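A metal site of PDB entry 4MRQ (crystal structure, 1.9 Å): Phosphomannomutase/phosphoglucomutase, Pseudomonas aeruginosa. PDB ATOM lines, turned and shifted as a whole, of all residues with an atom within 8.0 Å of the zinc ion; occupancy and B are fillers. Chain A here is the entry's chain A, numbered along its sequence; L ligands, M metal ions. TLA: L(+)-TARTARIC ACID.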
ATOM      1  N   THR A  79      21.452 -23.745  -6.067  1.00  0.00           N
ATOM      2  CA  THR A  79      20.192 -23.258  -5.479  1.00  0.00           C
ATOM      3  C   THR A  79      20.287 -21.912  -4.725  1.00  0.00           C
ATOM      4  O   THR A  79      19.480 -20.999  -4.971  1.00  0.00           O
ATOM      5  CB  THR A  79      19.579 -24.362  -4.588  1.00  0.00           C
ATOM      6  OG1 THR A  79      19.157 -25.435  -5.426  1.00  0.00           O
ATOM      7  CG2 THR A  79      18.387 -23.830  -3.724  1.00  0.00           C
ATOM      8  N   PRO A  80      21.260 -21.749  -3.802  1.00  0.00           N
ATOM      9  CA  PRO A  80      21.246 -20.433  -3.116  1.00  0.00           C
ATOM     10  C   PRO A  80      21.595 -19.259  -4.012  1.00  0.00           C
ATOM     11  O   PRO A  80      21.339 -18.093  -3.632  1.00  0.00           O
ATOM     12  CB  PRO A  80      22.339 -20.580  -2.022  1.00  0.00           C
ATOM     13  CG  PRO A  80      23.244 -21.681  -2.555  1.00  0.00           C
ATOM     14  CD  PRO A  80      22.281 -22.654  -3.216  1.00  0.00           C
ATOM     15  N   TYR A  83      18.292 -18.319  -5.142  1.00  0.00           N
ATOM     16  CA  TYR A  83      17.709 -17.511  -4.054  1.00  0.00           C
ATOM     17  C   TYR A  83      18.269 -16.082  -4.013  1.00  0.00           C
ATOM     18  O   TYR A  83      17.541 -15.139  -3.769  1.00  0.00           O
ATOM     19  CB  TYR A  83      17.950 -18.159  -2.688  1.00  0.00           C
ATOM     20  CG  TYR A  83      17.265 -19.510  -2.471  1.00  0.00           C
ATOM     21  CD1 TYR A  83      17.737 -20.375  -1.493  1.00  0.00           C
ATOM     22  CD2 TYR A  83      16.161 -19.912  -3.228  1.00  0.00           C
ATOM     23  CE1 TYR A  83      17.146 -21.616  -1.271  1.00  0.00           C
ATOM     24  CE2 TYR A  83      15.548 -21.154  -3.029  1.00  0.00           C
ATOM     25  CZ  TYR A  83      16.034 -22.003  -2.044  1.00  0.00           C
ATOM     26  OH  TYR A  83      15.436 -23.241  -1.816  1.00  0.00           O
ATOM     27  N   THR A  98      15.628 -28.249  -9.746  1.00  0.00           N
ATOM     28  CA  THR A  98      16.663 -29.086  -9.116  1.00  0.00           C
ATOM     29  C   THR A  98      16.090 -30.365  -8.574  1.00  0.00           C
ATOM     30  O   THR A  98      14.944 -30.399  -8.120  1.00  0.00           O
ATOM     31  CB  THR A  98      17.425 -28.336  -7.963  1.00  0.00           C
ATOM     32  OG1 THR A  98      18.429 -29.204  -7.411  1.00  0.00           O
ATOM     33  CG2 THR A  98      16.468 -27.887  -6.848  1.00  0.00           C
ATOM     34  N   GLY A  99      16.919 -31.414  -8.576  1.00  0.00           N
ATOM     35  CA  GLY A  99      16.590 -32.673  -7.939  1.00  0.00           C
ATOM     36  C   GLY A  99      17.453 -32.907  -6.699  1.00  0.00           C
ATOM     37  O   GLY A  99      17.509 -34.027  -6.191  1.00  0.00           O
ATOM     38  N   SER A 100      18.118 -31.832  -6.241  1.00  0.00           N
ATOM     39  CA  SER A 100      18.865 -31.804  -4.981  1.00  0.00           C
ATOM     40  C   SER A 100      19.994 -32.814  -4.900  1.00  0.00           C
ATOM     41  O   SER A 100      20.967 -32.711  -5.639  1.00  0.00           O
ATOM     42  CB  SER A 100      17.930 -31.964  -3.785  1.00  0.00           C
ATOM     43  OG  SER A 100      16.882 -31.010  -3.832  1.00  0.00           O
ATOM     44  N   HIS A 101      19.850 -33.783  -4.004  1.00  0.00           N
ATOM     45  CA  HIS A 101      20.889 -34.784  -3.719  1.00  0.00           C
ATOM     46  C   HIS A 101      20.540 -36.142  -4.309  1.00  0.00           C
ATOM     47  O   HIS A 101      21.302 -37.092  -4.154  1.00  0.00           O
ATOM     48  CB  HIS A 101      21.066 -34.923  -2.206  1.00  0.00           C
ATOM     49  CG  HIS A 101      19.893 -35.574  -1.524  1.00  0.00           C
ATOM     50  ND1 HIS A 101      18.615 -35.059  -1.585  1.00  0.00           N
ATOM     51  CD2 HIS A 101      19.811 -36.718  -0.801  1.00  0.00           C
ATOM     52  CE1 HIS A 101      17.801 -35.846  -0.907  1.00  0.00           C
ATOM     53  NE2 HIS A 101      18.503 -36.858  -0.424  1.00  0.00           N
ATOM     54  N   ASN A 102      19.406 -36.229  -4.997  1.00  0.00           N
ATOM     55  CA  ASN A 102      18.863 -37.531  -5.452  1.00  0.00           C
ATOM     56  C   ASN A 102      19.570 -38.082  -6.691  1.00  0.00           C
ATOM     57  O   ASN A 102      20.323 -37.331  -7.342  1.00  0.00           O
ATOM     58  CB  ASN A 102      17.350 -37.376  -5.705  1.00  0.00           C
ATOM     59  CG  ASN A 102      16.598 -37.064  -4.422  1.00  0.00           C
ATOM     60  OD1 ASN A 102      16.618 -37.843  -3.484  1.00  0.00           O
ATOM     61  ND2 ASN A 102      15.958 -35.912  -4.374  1.00  0.00           N
ATOM     62  N   LYS A 110      12.212 -25.841  -6.547  1.00  0.00           N
ATOM     63  CA  LYS A 110      12.091 -25.167  -5.253  1.00  0.00           C
ATOM     64  C   LYS A 110      11.648 -23.753  -5.598  1.00  0.00           C
ATOM     65  O   LYS A 110      12.165 -23.160  -6.575  1.00  0.00           O
ATOM     66  CB  LYS A 110      13.417 -25.160  -4.482  1.00  0.00           C
ATOM     67  CG  LYS A 110      13.914 -26.566  -4.173  1.00  0.00           C
ATOM     68  CD  LYS A 110      15.274 -26.599  -3.486  1.00  0.00           C
ATOM     69  CE  LYS A 110      15.581 -28.072  -3.194  1.00  0.00           C
ATOM     70  NZ  LYS A 110      16.873 -28.331  -2.477  1.00  0.00           N
ATOM     71  N   PRO A 207      25.921 -36.787  -4.213  1.00  0.00           N
ATOM     72  CA  PRO A 207      26.268 -35.566  -3.472  1.00  0.00           C
ATOM     73  C   PRO A 207      25.300 -35.296  -2.289  1.00  0.00           C
ATOM     74  O   PRO A 207      24.391 -34.461  -2.366  1.00  0.00           O
ATOM     75  CB  PRO A 207      26.229 -34.502  -4.556  1.00  0.00           C
ATOM     76  CG  PRO A 207      25.239 -34.996  -5.531  1.00  0.00           C
ATOM     77  CD  PRO A 207      25.314 -36.497  -5.529  1.00  0.00           C
ATOM     78  N   PRO A 209      25.953 -34.950   1.703  1.00  0.00           N
ATOM     79  CA  PRO A 209      26.919 -34.964   2.788  1.00  0.00           C
ATOM     80  C   PRO A 209      26.320 -35.340   4.156  1.00  0.00           C
ATOM     81  O   PRO A 209      27.057 -35.403   5.130  1.00  0.00           O
ATOM     82  CB  PRO A 209      27.443 -33.537   2.807  1.00  0.00           C
ATOM     83  CG  PRO A 209      26.333 -32.708   2.238  1.00  0.00           C
ATOM     84  CD  PRO A 209      25.723 -33.590   1.180  1.00  0.00           C
ATOM     85  N   PHE A 233      29.672 -30.463  -0.248  1.00  0.00           N
ATOM     86  CA  PHE A 233      28.398 -29.817  -0.560  1.00  0.00           C
ATOM     87  C   PHE A 233      27.450 -30.858  -1.114  1.00  0.00           C
ATOM     88  O   PHE A 233      27.892 -31.830  -1.733  1.00  0.00           O
ATOM     89  CB  PHE A 233      28.636 -28.712  -1.600  1.00  0.00           C
ATOM     90  CG  PHE A 233      29.501 -27.615  -1.080  1.00  0.00           C
ATOM     91  CD1 PHE A 233      28.964 -26.634  -0.233  1.00  0.00           C
ATOM     92  CD2 PHE A 233      30.887 -27.615  -1.301  1.00  0.00           C
ATOM     93  CE1 PHE A 233      29.762 -25.630   0.288  1.00  0.00           C
ATOM     94  CE2 PHE A 233      31.709 -26.633  -0.761  1.00  0.00           C
ATOM     95  CZ  PHE A 233      31.153 -25.627   0.027  1.00  0.00           C
ATOM     96  N   ASP A 234      26.149 -30.662  -0.893  1.00  0.00           N
ATOM     97  CA  ASP A 234      25.158 -31.473  -1.563  1.00  0.00           C
ATOM     98  C   ASP A 234      24.993 -31.063  -3.032  1.00  0.00           C
ATOM     99  O   ASP A 234      25.647 -30.117  -3.510  1.00  0.00           O
ATOM    100  CB  ASP A 234      23.816 -31.514  -0.767  1.00  0.00           C
ATOM    101  CG  ASP A 234      22.875 -30.331  -1.061  1.00  0.00           C
ATOM    102  OD1 ASP A 234      23.375 -29.233  -1.374  1.00  0.00           O
ATOM    103  OD2 ASP A 234      21.634 -30.532  -0.964  1.00  0.00           O
ATOM    104  N   GLY A 235      24.138 -31.788  -3.750  1.00  0.00           N
ATOM    105  CA  GLY A 235      24.025 -31.630  -5.234  1.00  0.00           C
ATOM    106  C   GLY A 235      23.765 -30.223  -5.748  1.00  0.00           C
ATOM    107  O   GLY A 235      24.351 -29.806  -6.771  1.00  0.00           O
ATOM    108  N   ASP A 236      22.905 -29.488  -5.036  1.00  0.00           N
ATOM    109  CA  ASP A 236      22.484 -28.151  -5.446  1.00  0.00           C
ATOM    110  C   ASP A 236      23.099 -26.995  -4.624  1.00  0.00           C
ATOM    111  O   ASP A 236      22.811 -25.817  -4.901  1.00  0.00           O
ATOM    112  CB  ASP A 236      20.943 -28.045  -5.570  1.00  0.00           C
ATOM    113  CG  ASP A 236      20.181 -28.259  -4.216  1.00  0.00           C
ATOM    114  OD1 ASP A 236      19.124 -27.621  -3.998  1.00  0.00           O
ATOM    115  OD2 ASP A 236      20.586 -29.121  -3.445  1.00  0.00           O
ATOM    116  N   GLY A 237      23.899 -27.338  -3.613  1.00  0.00           N
ATOM    117  CA  GLY A 237      24.681 -26.306  -2.835  1.00  0.00           C
ATOM    118  C   GLY A 237      23.957 -25.615  -1.675  1.00  0.00           C
ATOM    119  O   GLY A 237      24.497 -24.639  -1.108  1.00  0.00           O
ATOM    120  N   ASP A 238      22.739 -26.060  -1.311  1.00  0.00           N
ATOM    121  CA  ASP A 238      22.058 -25.405  -0.181  1.00  0.00           C
ATOM    122  C   ASP A 238      22.432 -26.058   1.159  1.00  0.00           C
ATOM    123  O   ASP A 238      21.982 -25.592   2.220  1.00  0.00           O
ATOM    124  CB  ASP A 238      20.527 -25.311  -0.395  1.00  0.00           C
ATOM    125  CG  ASP A 238      19.882 -26.666  -0.677  1.00  0.00           C
ATOM    126  OD1 ASP A 238      20.609 -27.711  -0.726  1.00  0.00           O
ATOM    127  OD2 ASP A 238      18.662 -26.706  -0.886  1.00  0.00           O
ATOM    128  N   ARG A 239      23.238 -27.122   1.109  1.00  0.00           N
ATOM    129  CA  ARG A 239      23.708 -27.835   2.319  1.00  0.00           C
ATOM    130  C   ARG A 239      25.182 -28.079   2.269  1.00  0.00           C
ATOM    131  O   ARG A 239      25.739 -28.261   1.179  1.00  0.00           O
ATOM    132  CB  ARG A 239      23.063 -29.216   2.471  1.00  0.00           C
ATOM    133  CG  ARG A 239      21.585 -29.190   2.689  1.00  0.00           C
ATOM    134  CD  ARG A 239      21.155 -30.536   3.214  1.00  0.00           C
ATOM    135  NE  ARG A 239      20.974 -31.520   2.165  1.00  0.00           N
ATOM    136  CZ  ARG A 239      21.529 -32.740   2.194  1.00  0.00           C
ATOM    137  NH1 ARG A 239      22.286 -33.078   3.220  1.00  0.00           N
ATOM    138  NH2 ARG A 239      21.277 -33.623   1.222  1.00  0.00           N
ATOM    139  N   VAL A 240      25.800 -28.125   3.444  1.00  0.00           N
ATOM    140  CA  VAL A 240      27.264 -28.315   3.525  1.00  0.00           C
ATOM    141  C   VAL A 240      27.572 -29.296   4.670  1.00  0.00           C
ATOM    142  O   VAL A 240      26.912 -29.271   5.708  1.00  0.00           O
ATOM    143  CB  VAL A 240      27.999 -26.951   3.745  1.00  0.00           C
ATOM    144  CG1 VAL A 240      27.553 -26.290   5.056  1.00  0.00           C
ATOM    145  CG2 VAL A 240      29.516 -27.086   3.662  1.00  0.00           C
ATOM    146  N   HIS A 300      13.409 -27.327   5.604  1.00  0.00           N
ATOM    147  CA  HIS A 300      14.066 -26.094   5.138  1.00  0.00           C
ATOM    148  C   HIS A 300      13.143 -24.893   5.098  1.00  0.00           C
ATOM    149  O   HIS A 300      13.456 -23.856   5.703  1.00  0.00           O
ATOM    150  CB  HIS A 300      14.881 -26.281   3.806  1.00  0.00           C
ATOM    151  CG  HIS A 300      14.108 -26.005   2.550  1.00  0.00           C
ATOM    152  ND1 HIS A 300      13.372 -26.978   1.883  1.00  0.00           N
ATOM    153  CD2 HIS A 300      13.956 -24.865   1.828  1.00  0.00           C
ATOM    154  CE1 HIS A 300      12.802 -26.437   0.812  1.00  0.00           C
ATOM    155  NE2 HIS A 300      13.144 -25.162   0.754  1.00  0.00           N
ATOM    156  N   SER A 319      20.035 -31.535   9.007  1.00  0.00           N
ATOM    157  CA  SER A 319      20.456 -32.088   7.713  1.00  0.00           C
ATOM    158  C   SER A 319      21.521 -31.231   7.008  1.00  0.00           C
ATOM    159  O   SER A 319      22.113 -31.636   6.007  1.00  0.00           O
ATOM    160  CB  SER A 319      19.250 -32.427   6.807  1.00  0.00           C
ATOM    161  OG  SER A 319      18.746 -31.266   6.148  1.00  0.00           O
ATOM    162  N   HIS A 321      21.163 -27.534   6.389  1.00  0.00           N
ATOM    163  CA  HIS A 321      20.766 -26.251   5.847  1.00  0.00           C
ATOM    164  C   HIS A 321      21.090 -25.246   6.961  1.00  0.00           C
ATOM    165  O   HIS A 321      20.636 -25.410   8.130  1.00  0.00           O
ATOM    166  CB  HIS A 321      19.275 -26.175   5.547  1.00  0.00           C
ATOM    167  CG  HIS A 321      18.818 -27.074   4.415  1.00  0.00           C
ATOM    168  ND1 HIS A 321      18.674 -26.631   3.119  1.00  0.00           N
ATOM    169  CD2 HIS A 321      18.396 -28.357   4.423  1.00  0.00           C
ATOM    170  CE1 HIS A 321      18.218 -27.615   2.372  1.00  0.00           C
ATOM    171  NE2 HIS A 321      18.057 -28.680   3.127  1.00  0.00           N
ATOM    172  N   ASP A 332      18.915 -20.433   3.073  1.00  0.00           N
ATOM    173  CA  ASP A 332      19.925 -21.448   3.334  1.00  0.00           C
ATOM    174  C   ASP A 332      20.941 -21.467   2.196  1.00  0.00           C
ATOM    175  O   ASP A 332      20.561 -21.338   1.020  1.00  0.00           O
ATOM    176  CB  ASP A 332      19.310 -22.818   3.527  1.00  0.00           C
ATOM    177  CG  ASP A 332      18.197 -23.122   2.521  1.00  0.00           C
ATOM    178  OD1 ASP A 332      18.090 -24.274   2.105  1.00  0.00           O
ATOM    179  OD2 ASP A 332      17.392 -22.228   2.150  1.00  0.00           O
HETATM  180  O1  TLA L   1      15.925 -34.260   1.209  1.00  0.00           O
HETATM  181  O11 TLA L   1      14.605 -32.925   0.093  1.00  0.00           O
HETATM  182  C1  TLA L   1      15.742 -33.298   0.428  1.00  0.00           C
HETATM  183  C2  TLA L   1      16.940 -32.570  -0.128  1.00  0.00           C
HETATM  184  O2  TLA L   1      18.171 -33.049   0.473  1.00  0.00           O
HETATM  185  C3  TLA L   1      16.800 -31.083   0.140  1.00  0.00           C
HETATM  186  O3  TLA L   1      16.632 -30.859   1.571  1.00  0.00           O
HETATM  187  C4  TLA L   1      18.133 -30.506  -0.223  1.00  0.00           C
HETATM  188  O4  TLA L   1      18.935 -30.339   0.687  1.00  0.00           O
HETATM  189  O41 TLA L   1      18.383 -30.199  -1.396  1.00  0.00           O
HETATM  190 ZN    ZN M   1      20.191 -29.405  -1.437  1.00  0.00          ZN
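The zinc ion is bound by the side-chain carboxylate (OD1) of Asp 238 (1.9 Å). The side-chain carboxylate (OD2) of Asp 234 is bound to the zinc ion. The zinc ion is bound by O41 of the ligand (2.0 Å). The side-chain carboxylate (OD2) of Asp 236 binds the zinc ion (2.1 Å). The zinc ion has four donor atoms within binding distance. Slightly farther from the zinc ion lies O4 of the ligand (2.6 Å).
NZ of Lys 110 is in salt-bridge range of OD1 of Asp 236 (2.8 Å). The side-chain hydroxyl of Thr 79 sits at hydrogen-bond distance from the side-chain carboxylate of Asp 236 (2.6 Å). The side-chain hydroxyl (OG) of Ser 100 sits at hydrogen-bond distance from the side-chain amino group (NZ) of Lys 110, at 3.0 Å. The backbone carbonyl oxygen of Arg 239 lies within hydrogen-bond range of the backbone NH of Asp 234 (3.2 Å). OD1 of Asp 234 lies within hydrogen-bond range of N of Gly 237, 3.0 Å away. The side-chain carboxylate (OD2) of Asp 238 lies within salt-bridge range of the side-chain amino group (NZ) of Lys 110 (2.9 Å).
Residues that only touch the zinc ion: Lys 110 (3.6 Å).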
